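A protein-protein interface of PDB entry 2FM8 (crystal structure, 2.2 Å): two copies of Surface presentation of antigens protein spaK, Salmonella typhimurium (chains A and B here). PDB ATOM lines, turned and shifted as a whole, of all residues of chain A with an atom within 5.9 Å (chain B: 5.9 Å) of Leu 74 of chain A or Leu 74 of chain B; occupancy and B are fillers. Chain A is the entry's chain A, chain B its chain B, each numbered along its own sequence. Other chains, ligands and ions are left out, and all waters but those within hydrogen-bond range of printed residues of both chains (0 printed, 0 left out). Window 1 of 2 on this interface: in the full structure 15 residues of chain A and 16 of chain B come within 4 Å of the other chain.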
ATOM      1  N   LEU A  66      10.918  15.859  -7.485  1.00  0.00           N
ATOM      2  CA  LEU A  66      10.857  15.486  -6.067  1.00  0.00           C
ATOM      3  C   LEU A  66      12.128  15.889  -5.272  1.00  0.00           C
ATOM      4  O   LEU A  66      12.052  16.215  -4.090  1.00  0.00           O
ATOM      5  CB  LEU A  66      10.547  14.011  -5.921  1.00  0.00           C
ATOM      6  CG  LEU A  66      10.240  13.461  -4.515  1.00  0.00           C
ATOM      7  CD1 LEU A  66       9.016  14.105  -3.859  1.00  0.00           C
ATOM      8  CD2 LEU A  66      10.047  11.979  -4.605  1.00  0.00           C
ATOM      9  N   ARG A  69      11.268  19.318  -4.203  1.00  0.00           N
ATOM     10  CA  ARG A  69       9.924  19.556  -3.656  1.00  0.00           C
ATOM     11  C   ARG A  69       9.475  18.580  -2.592  1.00  0.00           C
ATOM     12  O   ARG A  69       8.274  18.515  -2.258  1.00  0.00           O
ATOM     13  CB  ARG A  69       8.913  19.579  -4.795  1.00  0.00           C
ATOM     14  CG  ARG A  69       8.526  20.965  -5.184  1.00  0.00           C
ATOM     15  CD  ARG A  69       9.216  21.423  -6.377  1.00  0.00           C
ATOM     16  NE  ARG A  69       9.191  22.880  -6.427  1.00  0.00           N
ATOM     17  CZ  ARG A  69       9.092  23.598  -7.555  1.00  0.00           C
ATOM     18  NH1 ARG A  69       8.995  22.997  -8.782  1.00  0.00           N
ATOM     19  NH2 ARG A  69       9.075  24.947  -7.453  1.00  0.00           N
ATOM     20  N   ALA A  70      10.416  17.814  -2.043  1.00  0.00           N
ATOM     21  CA  ALA A  70      10.062  16.775  -1.086  1.00  0.00           C
ATOM     22  C   ALA A  70       9.392  17.300   0.181  1.00  0.00           C
ATOM     23  O   ALA A  70       8.480  16.651   0.698  1.00  0.00           O
ATOM     24  CB  ALA A  70      11.253  15.913  -0.734  1.00  0.00           C
ATOM     25  N   TYR A  71       9.791  18.467   0.667  1.00  0.00           N
ATOM     26  CA  TYR A  71       9.141  19.026   1.859  1.00  0.00           C
ATOM     27  C   TYR A  71       7.668  19.377   1.651  1.00  0.00           C
ATOM     28  O   TYR A  71       6.798  19.051   2.460  1.00  0.00           O
ATOM     29  CB  TYR A  71       9.879  20.284   2.281  1.00  0.00           C
ATOM     30  CG  TYR A  71       9.356  20.930   3.532  1.00  0.00           C
ATOM     31  CD1 TYR A  71       9.142  20.181   4.713  1.00  0.00           C
ATOM     32  CD2 TYR A  71       9.077  22.291   3.547  1.00  0.00           C
ATOM     33  CE1 TYR A  71       8.670  20.795   5.870  1.00  0.00           C
ATOM     34  CE2 TYR A  71       8.618  22.906   4.681  1.00  0.00           C
ATOM     35  CZ  TYR A  71       8.424  22.171   5.839  1.00  0.00           C
ATOM     36  OH  TYR A  71       8.004  22.851   6.943  1.00  0.00           O
ATOM     37  N   GLU A  72       7.395  20.066   0.550  1.00  0.00           N
ATOM     38  CA  GLU A  72       6.022  20.396   0.182  1.00  0.00           C
ATOM     39  C   GLU A  72       5.182  19.124  -0.007  1.00  0.00           C
ATOM     40  O   GLU A  72       4.001  19.073   0.356  1.00  0.00           O
ATOM     41  CB  GLU A  72       6.028  21.278  -1.082  1.00  0.00           C
ATOM     42  CG  GLU A  72       4.644  21.509  -1.689  1.00  0.00           C
ATOM     43  CD  GLU A  72       4.688  22.490  -2.877  1.00  0.00           C
ATOM     44  OE1 GLU A  72       5.606  23.308  -2.932  1.00  0.00           O
ATOM     45  OE2 GLU A  72       3.818  22.432  -3.744  1.00  0.00           O
ATOM     46  N   ILE A  73       5.789  18.098  -0.572  1.00  0.00           N
ATOM     47  CA  ILE A  73       5.090  16.842  -0.787  1.00  0.00           C
ATOM     48  C   ILE A  73       4.788  16.170   0.542  1.00  0.00           C
ATOM     49  O   ILE A  73       3.667  15.725   0.784  1.00  0.00           O
ATOM     50  CB  ILE A  73       5.886  15.941  -1.743  1.00  0.00           C
ATOM     51  CG1 ILE A  73       5.855  16.534  -3.174  1.00  0.00           C
ATOM     52  CG2 ILE A  73       5.389  14.494  -1.728  1.00  0.00           C
ATOM     53  CD1 ILE A  73       4.497  16.443  -3.884  1.00  0.00           C
ATOM     54  N   LEU A  74       5.777  16.133   1.426  1.00  0.00           N
ATOM     55  CA  LEU A  74       5.568  15.573   2.757  1.00  0.00           C
ATOM     56  C   LEU A  74       4.477  16.306   3.580  1.00  0.00           C
ATOM     57  O   LEU A  74       3.657  15.656   4.233  1.00  0.00           O
ATOM     58  CB  LEU A  74       6.879  15.509   3.501  1.00  0.00           C
ATOM     59  CG  LEU A  74       7.458  14.185   3.987  1.00  0.00           C
ATOM     60  CD1 LEU A  74       7.030  12.950   3.263  1.00  0.00           C
ATOM     61  CD2 LEU A  74       8.975  14.308   4.052  1.00  0.00           C
ATOM     62  N   MET A  75       4.474  17.642   3.552  1.00  0.00           N
ATOM     63  CA  MET A  75       3.420  18.410   4.220  1.00  0.00           C
ATOM     64  C   MET A  75       2.063  18.039   3.700  1.00  0.00           C
ATOM     65  O   MET A  75       1.107  17.888   4.475  1.00  0.00           O
ATOM     66  CB  MET A  75       3.552  19.909   3.956  1.00  0.00           C
ATOM     67  CG  MET A  75       4.869  20.547   4.264  1.00  0.00           C
ATOM     68  SD  MET A  75       4.682  21.762   5.578  1.00  0.00           S
ATOM     69  CE  MET A  75       4.813  20.359   6.673  1.00  0.00           C
ATOM     70  N   THR A  76       1.961  17.940   2.373  1.00  0.00           N
ATOM     71  CA  THR A  76       0.728  17.515   1.743  1.00  0.00           C
ATOM     72  C   THR A  76       0.282  16.109   2.233  1.00  0.00           C
ATOM     73  O   THR A  76      -0.871  15.904   2.590  1.00  0.00           O
ATOM     74  CB  THR A  76       0.828  17.569   0.200  1.00  0.00           C
ATOM     75  OG1 THR A  76       1.416  18.814  -0.222  1.00  0.00           O
ATOM     76  CG2 THR A  76      -0.546  17.446  -0.424  1.00  0.00           C
ATOM     77  N   ILE A  77       1.186  15.145   2.209  1.00  0.00           N
ATOM     78  CA  ILE A  77       0.928  13.809   2.746  1.00  0.00           C
ATOM     79  C   ILE A  77       0.430  13.880   4.215  1.00  0.00           C
ATOM     80  O   ILE A  77      -0.606  13.273   4.590  1.00  0.00           O
ATOM     81  CB  ILE A  77       2.223  12.913   2.630  1.00  0.00           C
ATOM     82  CG1 ILE A  77       2.483  12.487   1.160  1.00  0.00           C
ATOM     83  CG2 ILE A  77       2.140  11.666   3.464  1.00  0.00           C
ATOM     84  CD1 ILE A  77       1.421  11.562   0.574  1.00  0.00           C
ATOM     85  N   MET A  78       1.132  14.661   5.023  1.00  0.00           N
ATOM     86  CA  MET A  78       0.822  14.727   6.456  1.00  0.00           C
ATOM     87  C   MET A  78      -0.512  15.378   6.786  1.00  0.00           C
ATOM     88  O   MET A  78      -1.036  15.171   7.891  1.00  0.00           O
ATOM     89  CB  MET A  78       1.940  15.386   7.227  1.00  0.00           C
ATOM     90  CG  MET A  78       3.167  14.537   7.186  1.00  0.00           C
ATOM     91  SD  MET A  78       4.549  15.260   8.055  1.00  0.00           S
ATOM     92  CE  MET A  78       3.951  15.173   9.744  1.00  0.00           C
ATOM     93  N   GLU A  79      -1.077  16.127   5.828  1.00  0.00           N
ATOM     94  CA  GLU A  79      -2.387  16.709   6.033  1.00  0.00           C
ATOM     95  C   GLU A  79      -3.504  15.638   6.067  1.00  0.00           C
ATOM     96  O   GLU A  79      -4.588  15.872   6.625  1.00  0.00           O
ATOM     97  CB  GLU A  79      -2.649  17.866   5.054  1.00  0.00           C
ATOM     98  CG  GLU A  79      -3.180  17.501   3.716  1.00  0.00           C
ATOM     99  CD  GLU A  79      -3.622  18.743   2.884  1.00  0.00           C
ATOM    100  OE1 GLU A  79      -2.953  19.817   3.020  1.00  0.00           O
ATOM    101  OE2 GLU A  79      -4.632  18.602   2.128  1.00  0.00           O
ATOM    102  N   LEU A  91       3.186   7.027  -1.220  1.00  0.00           N
ATOM    103  CA  LEU A  91       3.967   7.282  -2.416  1.00  0.00           C
ATOM    104  C   LEU A  91       4.784   6.057  -2.774  1.00  0.00           C
ATOM    105  O   LEU A  91       5.456   5.504  -1.943  1.00  0.00           O
ATOM    106  CB  LEU A  91       4.911   8.462  -2.209  1.00  0.00           C
ATOM    107  CG  LEU A  91       4.219   9.787  -1.977  1.00  0.00           C
ATOM    108  CD1 LEU A  91       5.242  10.803  -1.450  1.00  0.00           C
ATOM    109  CD2 LEU A  91       3.565  10.318  -3.240  1.00  0.00           C
ATOM    110  N   LEU B  66      13.071  17.508   9.711  1.00  0.00           N
ATOM    111  CA  LEU B  66      12.215  17.056   8.639  1.00  0.00           C
ATOM    112  C   LEU B  66      12.239  17.980   7.426  1.00  0.00           C
ATOM    113  O   LEU B  66      12.373  17.530   6.294  1.00  0.00           O
ATOM    114  CB  LEU B  66      10.778  16.912   9.155  1.00  0.00           C
ATOM    115  CG  LEU B  66       9.784  16.527   8.056  1.00  0.00           C
ATOM    116  CD1 LEU B  66       9.981  15.119   7.637  1.00  0.00           C
ATOM    117  CD2 LEU B  66       8.400  16.761   8.494  1.00  0.00           C
ATOM    118  N   ARG B  69      15.729  17.786   5.762  1.00  0.00           N
ATOM    119  CA  ARG B  69      16.103  16.486   5.182  1.00  0.00           C
ATOM    120  C   ARG B  69      14.921  15.722   4.630  1.00  0.00           C
ATOM    121  O   ARG B  69      14.927  14.506   4.567  1.00  0.00           O
ATOM    122  CB  ARG B  69      16.820  15.643   6.239  1.00  0.00           C
ATOM    123  CG  ARG B  69      18.050  16.357   6.802  1.00  0.00           C
ATOM    124  CD  ARG B  69      18.751  15.453   7.755  1.00  0.00           C
ATOM    125  NE  ARG B  69      19.856  16.133   8.420  1.00  0.00           N
ATOM    126  CZ  ARG B  69      20.412  15.715   9.547  1.00  0.00           C
ATOM    127  NH1 ARG B  69      19.953  14.643  10.177  1.00  0.00           N
ATOM    128  NH2 ARG B  69      21.409  16.400  10.058  1.00  0.00           N
ATOM    129  N   ALA B  70      13.922  16.452   4.176  1.00  0.00           N
ATOM    130  CA  ALA B  70      12.679  15.870   3.659  1.00  0.00           C
ATOM    131  C   ALA B  70      12.916  14.798   2.575  1.00  0.00           C
ATOM    132  O   ALA B  70      12.349  13.729   2.642  1.00  0.00           O
ATOM    133  CB  ALA B  70      11.779  17.010   3.114  1.00  0.00           C
ATOM    134  N   TYR B  71      13.769  15.091   1.596  1.00  0.00           N
ATOM    135  CA  TYR B  71      13.993  14.193   0.466  1.00  0.00           C
ATOM    136  C   TYR B  71      14.555  12.879   0.957  1.00  0.00           C
ATOM    137  O   TYR B  71      14.015  11.793   0.699  1.00  0.00           O
ATOM    138  CB  TYR B  71      14.944  14.844  -0.553  1.00  0.00           C
ATOM    139  CG  TYR B  71      15.293  13.939  -1.712  1.00  0.00           C
ATOM    140  CD1 TYR B  71      14.370  13.702  -2.741  1.00  0.00           C
ATOM    141  CD2 TYR B  71      16.530  13.296  -1.776  1.00  0.00           C
ATOM    142  CE1 TYR B  71      14.673  12.846  -3.803  1.00  0.00           C
ATOM    143  CE2 TYR B  71      16.850  12.436  -2.857  1.00  0.00           C
ATOM    144  CZ  TYR B  71      15.907  12.203  -3.854  1.00  0.00           C
ATOM    145  OH  TYR B  71      16.220  11.384  -4.931  1.00  0.00           O
ATOM    146  N   GLU B  72      15.624  12.992   1.731  1.00  0.00           N
ATOM    147  CA  GLU B  72      16.311  11.845   2.289  1.00  0.00           C
ATOM    148  C   GLU B  72      15.336  10.995   3.108  1.00  0.00           C
ATOM    149  O   GLU B  72      15.331   9.775   3.020  1.00  0.00           O
ATOM    150  CB  GLU B  72      17.465  12.342   3.196  1.00  0.00           C
ATOM    151  CG  GLU B  72      18.483  13.249   2.486  1.00  0.00           C
ATOM    152  CD  GLU B  72      18.309  14.793   2.688  1.00  0.00           C
ATOM    153  OE1 GLU B  72      17.301  15.363   2.244  1.00  0.00           O
ATOM    154  OE2 GLU B  72      19.254  15.448   3.237  1.00  0.00           O
ATOM    155  N   ILE B  73      14.514  11.651   3.918  1.00  0.00           N
ATOM    156  CA  ILE B  73      13.567  10.964   4.776  1.00  0.00           C
ATOM    157  C   ILE B  73      12.478  10.303   3.928  1.00  0.00           C
ATOM    158  O   ILE B  73      12.107   9.170   4.140  1.00  0.00           O
ATOM    159  CB  ILE B  73      12.960  11.950   5.815  1.00  0.00           C
ATOM    160  CG1 ILE B  73      14.017  12.333   6.882  1.00  0.00           C
ATOM    161  CG2 ILE B  73      11.769  11.341   6.500  1.00  0.00           C
ATOM    162  CD1 ILE B  73      13.670  13.620   7.665  1.00  0.00           C
ATOM    163  N   LEU B  74      11.983  11.016   2.941  1.00  0.00           N
ATOM    164  CA  LEU B  74      10.995  10.431   2.029  1.00  0.00           C
ATOM    165  C   LEU B  74      11.524   9.219   1.262  1.00  0.00           C
ATOM    166  O   LEU B  74      10.806   8.234   1.097  1.00  0.00           O
ATOM    167  CB  LEU B  74      10.482  11.510   1.067  1.00  0.00           C
ATOM    168  CG  LEU B  74       9.422  11.101   0.074  1.00  0.00           C
ATOM    169  CD1 LEU B  74       8.248  10.417   0.810  1.00  0.00           C
ATOM    170  CD2 LEU B  74       8.966  12.316  -0.689  1.00  0.00           C
ATOM    171  N   MET B  75      12.777   9.273   0.800  1.00  0.00           N
ATOM    172  CA  MET B  75      13.380   8.115   0.102  1.00  0.00           C
ATOM    173  C   MET B  75      13.431   6.843   0.983  1.00  0.00           C
ATOM    174  O   MET B  75      13.227   5.713   0.504  1.00  0.00           O
ATOM    175  CB  MET B  75      14.781   8.465  -0.406  1.00  0.00           C
ATOM    176  CG  MET B  75      14.813   9.471  -1.565  1.00  0.00           C
ATOM    177  SD  MET B  75      13.766   9.083  -2.984  1.00  0.00           S
ATOM    178  CE  MET B  75      12.300  10.022  -2.622  1.00  0.00           C
ATOM    179  N   THR B  76      13.676   7.042   2.280  1.00  0.00           N
ATOM    180  CA  THR B  76      13.721   5.917   3.216  1.00  0.00           C
ATOM    181  C   THR B  76      12.338   5.340   3.404  1.00  0.00           C
ATOM    182  O   THR B  76      12.172   4.116   3.408  1.00  0.00           O
ATOM    183  CB  THR B  76      14.281   6.350   4.560  1.00  0.00           C
ATOM    184  OG1 THR B  76      15.561   6.931   4.367  1.00  0.00           O
ATOM    185  CG2 THR B  76      14.433   5.192   5.484  1.00  0.00           C
ATOM    186  N   ILE B  77      11.340   6.219   3.549  1.00  0.00           N
ATOM    187  CA  ILE B  77       9.934   5.786   3.621  1.00  0.00           C
ATOM    188  C   ILE B  77       9.550   4.971   2.399  1.00  0.00           C
ATOM    189  O   ILE B  77       8.872   3.956   2.538  1.00  0.00           O
ATOM    190  CB  ILE B  77       8.991   6.962   3.734  1.00  0.00           C
ATOM    191  CG1 ILE B  77       9.051   7.530   5.125  1.00  0.00           C
ATOM    192  CG2 ILE B  77       7.493   6.558   3.423  1.00  0.00           C
ATOM    193  CD1 ILE B  77       8.436   8.881   5.149  1.00  0.00           C
ATOM    194  N   MET B  78       9.973   5.421   1.213  1.00  0.00           N
ATOM    195  CA  MET B  78       9.658   4.704  -0.024  1.00  0.00           C
ATOM    196  C   MET B  78      10.332   3.342  -0.174  1.00  0.00           C
ATOM    197  O   MET B  78       9.959   2.616  -1.033  1.00  0.00           O
ATOM    198  CB  MET B  78       9.925   5.571  -1.270  1.00  0.00           C
ATOM    199  CG  MET B  78       9.054   6.846  -1.321  1.00  0.00           C
ATOM    200  SD  MET B  78       9.347   7.911  -2.750  1.00  0.00           S
ATOM    201  CE  MET B  78       8.964   6.796  -4.091  1.00  0.00           C
ATOM    202  N   GLU B  79      11.317   3.000   0.652  1.00  0.00           N
ATOM    203  CA  GLU B  79      11.923   1.660   0.638  1.00  0.00           C
ATOM    204  C   GLU B  79      11.008   0.642   1.275  1.00  0.00           C
ATOM    205  O   GLU B  79      11.215  -0.544   1.127  1.00  0.00           O
ATOM    206  CB  GLU B  79      13.296   1.638   1.367  1.00  0.00           C
ATOM    207  CG  GLU B  79      14.401   2.386   0.600  1.00  0.00           C
ATOM    208  CD  GLU B  79      14.614   1.799  -0.780  1.00  0.00           C
ATOM    209  OE1 GLU B  79      14.695   0.575  -0.891  1.00  0.00           O
ATOM    210  OE2 GLU B  79      14.671   2.533  -1.764  1.00  0.00           O
ATOM    211  N   LEU B  91       4.387   9.021   8.517  1.00  0.00           N
ATOM    212  CA  LEU B  91       4.813  10.137   9.347  1.00  0.00           C
ATOM    213  C   LEU B  91       3.630  10.913   9.872  1.00  0.00           C
ATOM    214  O   LEU B  91       2.673  11.230   9.132  1.00  0.00           O
ATOM    215  CB  LEU B  91       5.676  11.085   8.558  1.00  0.00           C
ATOM    216  CG  LEU B  91       7.027  10.600   8.058  1.00  0.00           C
ATOM    217  CD1 LEU B  91       7.701  11.760   7.380  1.00  0.00           C
ATOM    218  CD2 LEU B  91       7.919  10.080   9.146  1.00  0.00           C
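Ala 70 of chain A touches Tyr 71 of chain B, and with the chains exchanged Tyr 71 of chain A touches Ala 70 of chain B. Leu 74 of chain A touches Ala 70 of chain B, but with the chains exchanged Ala 70 of chain A does not touch Leu 74 of chain B (4.3 Å). Leu 74 of chain A touches its own counterpart, Leu 74 of chain B. Leu 91 of chain A touches Leu 74 of chain B, but with the chains exchanged Leu 74 of chain A does not touch Leu 91 of chain B (4.2 Å). 13 positions are printed for both chains. Of the 12 pairs that touch across the chains among the printed residues, 8 have their exchanged pair printed and touching as well.
Leu 74 of chain A touches just these residues of chain B: Leu 66, Ala 70 and Leu 74. Of the printed residues of chain A, Leu 66 of chain B touches Leu 74. Of the printed residues of chain A, Leu 91 of chain B touches Met 78. Thr 76 of chain A touches none of the printed residues of chain B. Thr 76 of chain B touches none of the printed residues of chain A.
OH of Tyr 71 of chain A is in hydrogen-bond range of SD of Met 75 of chain A, at 3.8 Å.
Along chain A the printed residues that touch a printed residue of chain B span positions 66 to 91. Of the 13 printed residues of chain B, 7 touch a printed residue of chain A. Printed residues of chain B that touch a printed residue of chain A: Leu 66, Ala 70, Tyr 71, Leu 74, Met 75, Met 78 and Leu 91. Hydrophobic or aromatic side chains of chain B that line the printed part of chain A: Leu 66, Ala 70, Tyr 71, Leu 74, Met 75 and Met 78. Among the printed residues, 12 pairs touch across the chains.
Leu 66 of chain A touches Leu 74 of chain B. CE of Met 75 of chain B touches CD2 of Leu 66 of chain A (3.6 Å). Ala 70 of chain A touches Tyr 71 of chain B (CB to CA, 3.5 Å). CB of Ala 70 of chain B touches N of Tyr 71 of chain A (3.5 Å). CD2 of Leu 74 of chain A touches CD1 of Leu 66 of chain B, 3.8 Å away. O of Ala 70 of chain B touches CD2 of Leu 74 of chain A, at 3.7 Å. CD1 of Leu 74 of chain B touches CD1 of Leu 74 of chain A, 3.7 Å away. Met 78 of chain A touches Leu 91 of chain B (CG to O, 3.9 Å). Leu 74 of chain B touches Leu 91 of chain A. CG of Met 78 of chain B touches O of Leu 91 of chain A, 3.9 Å away.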
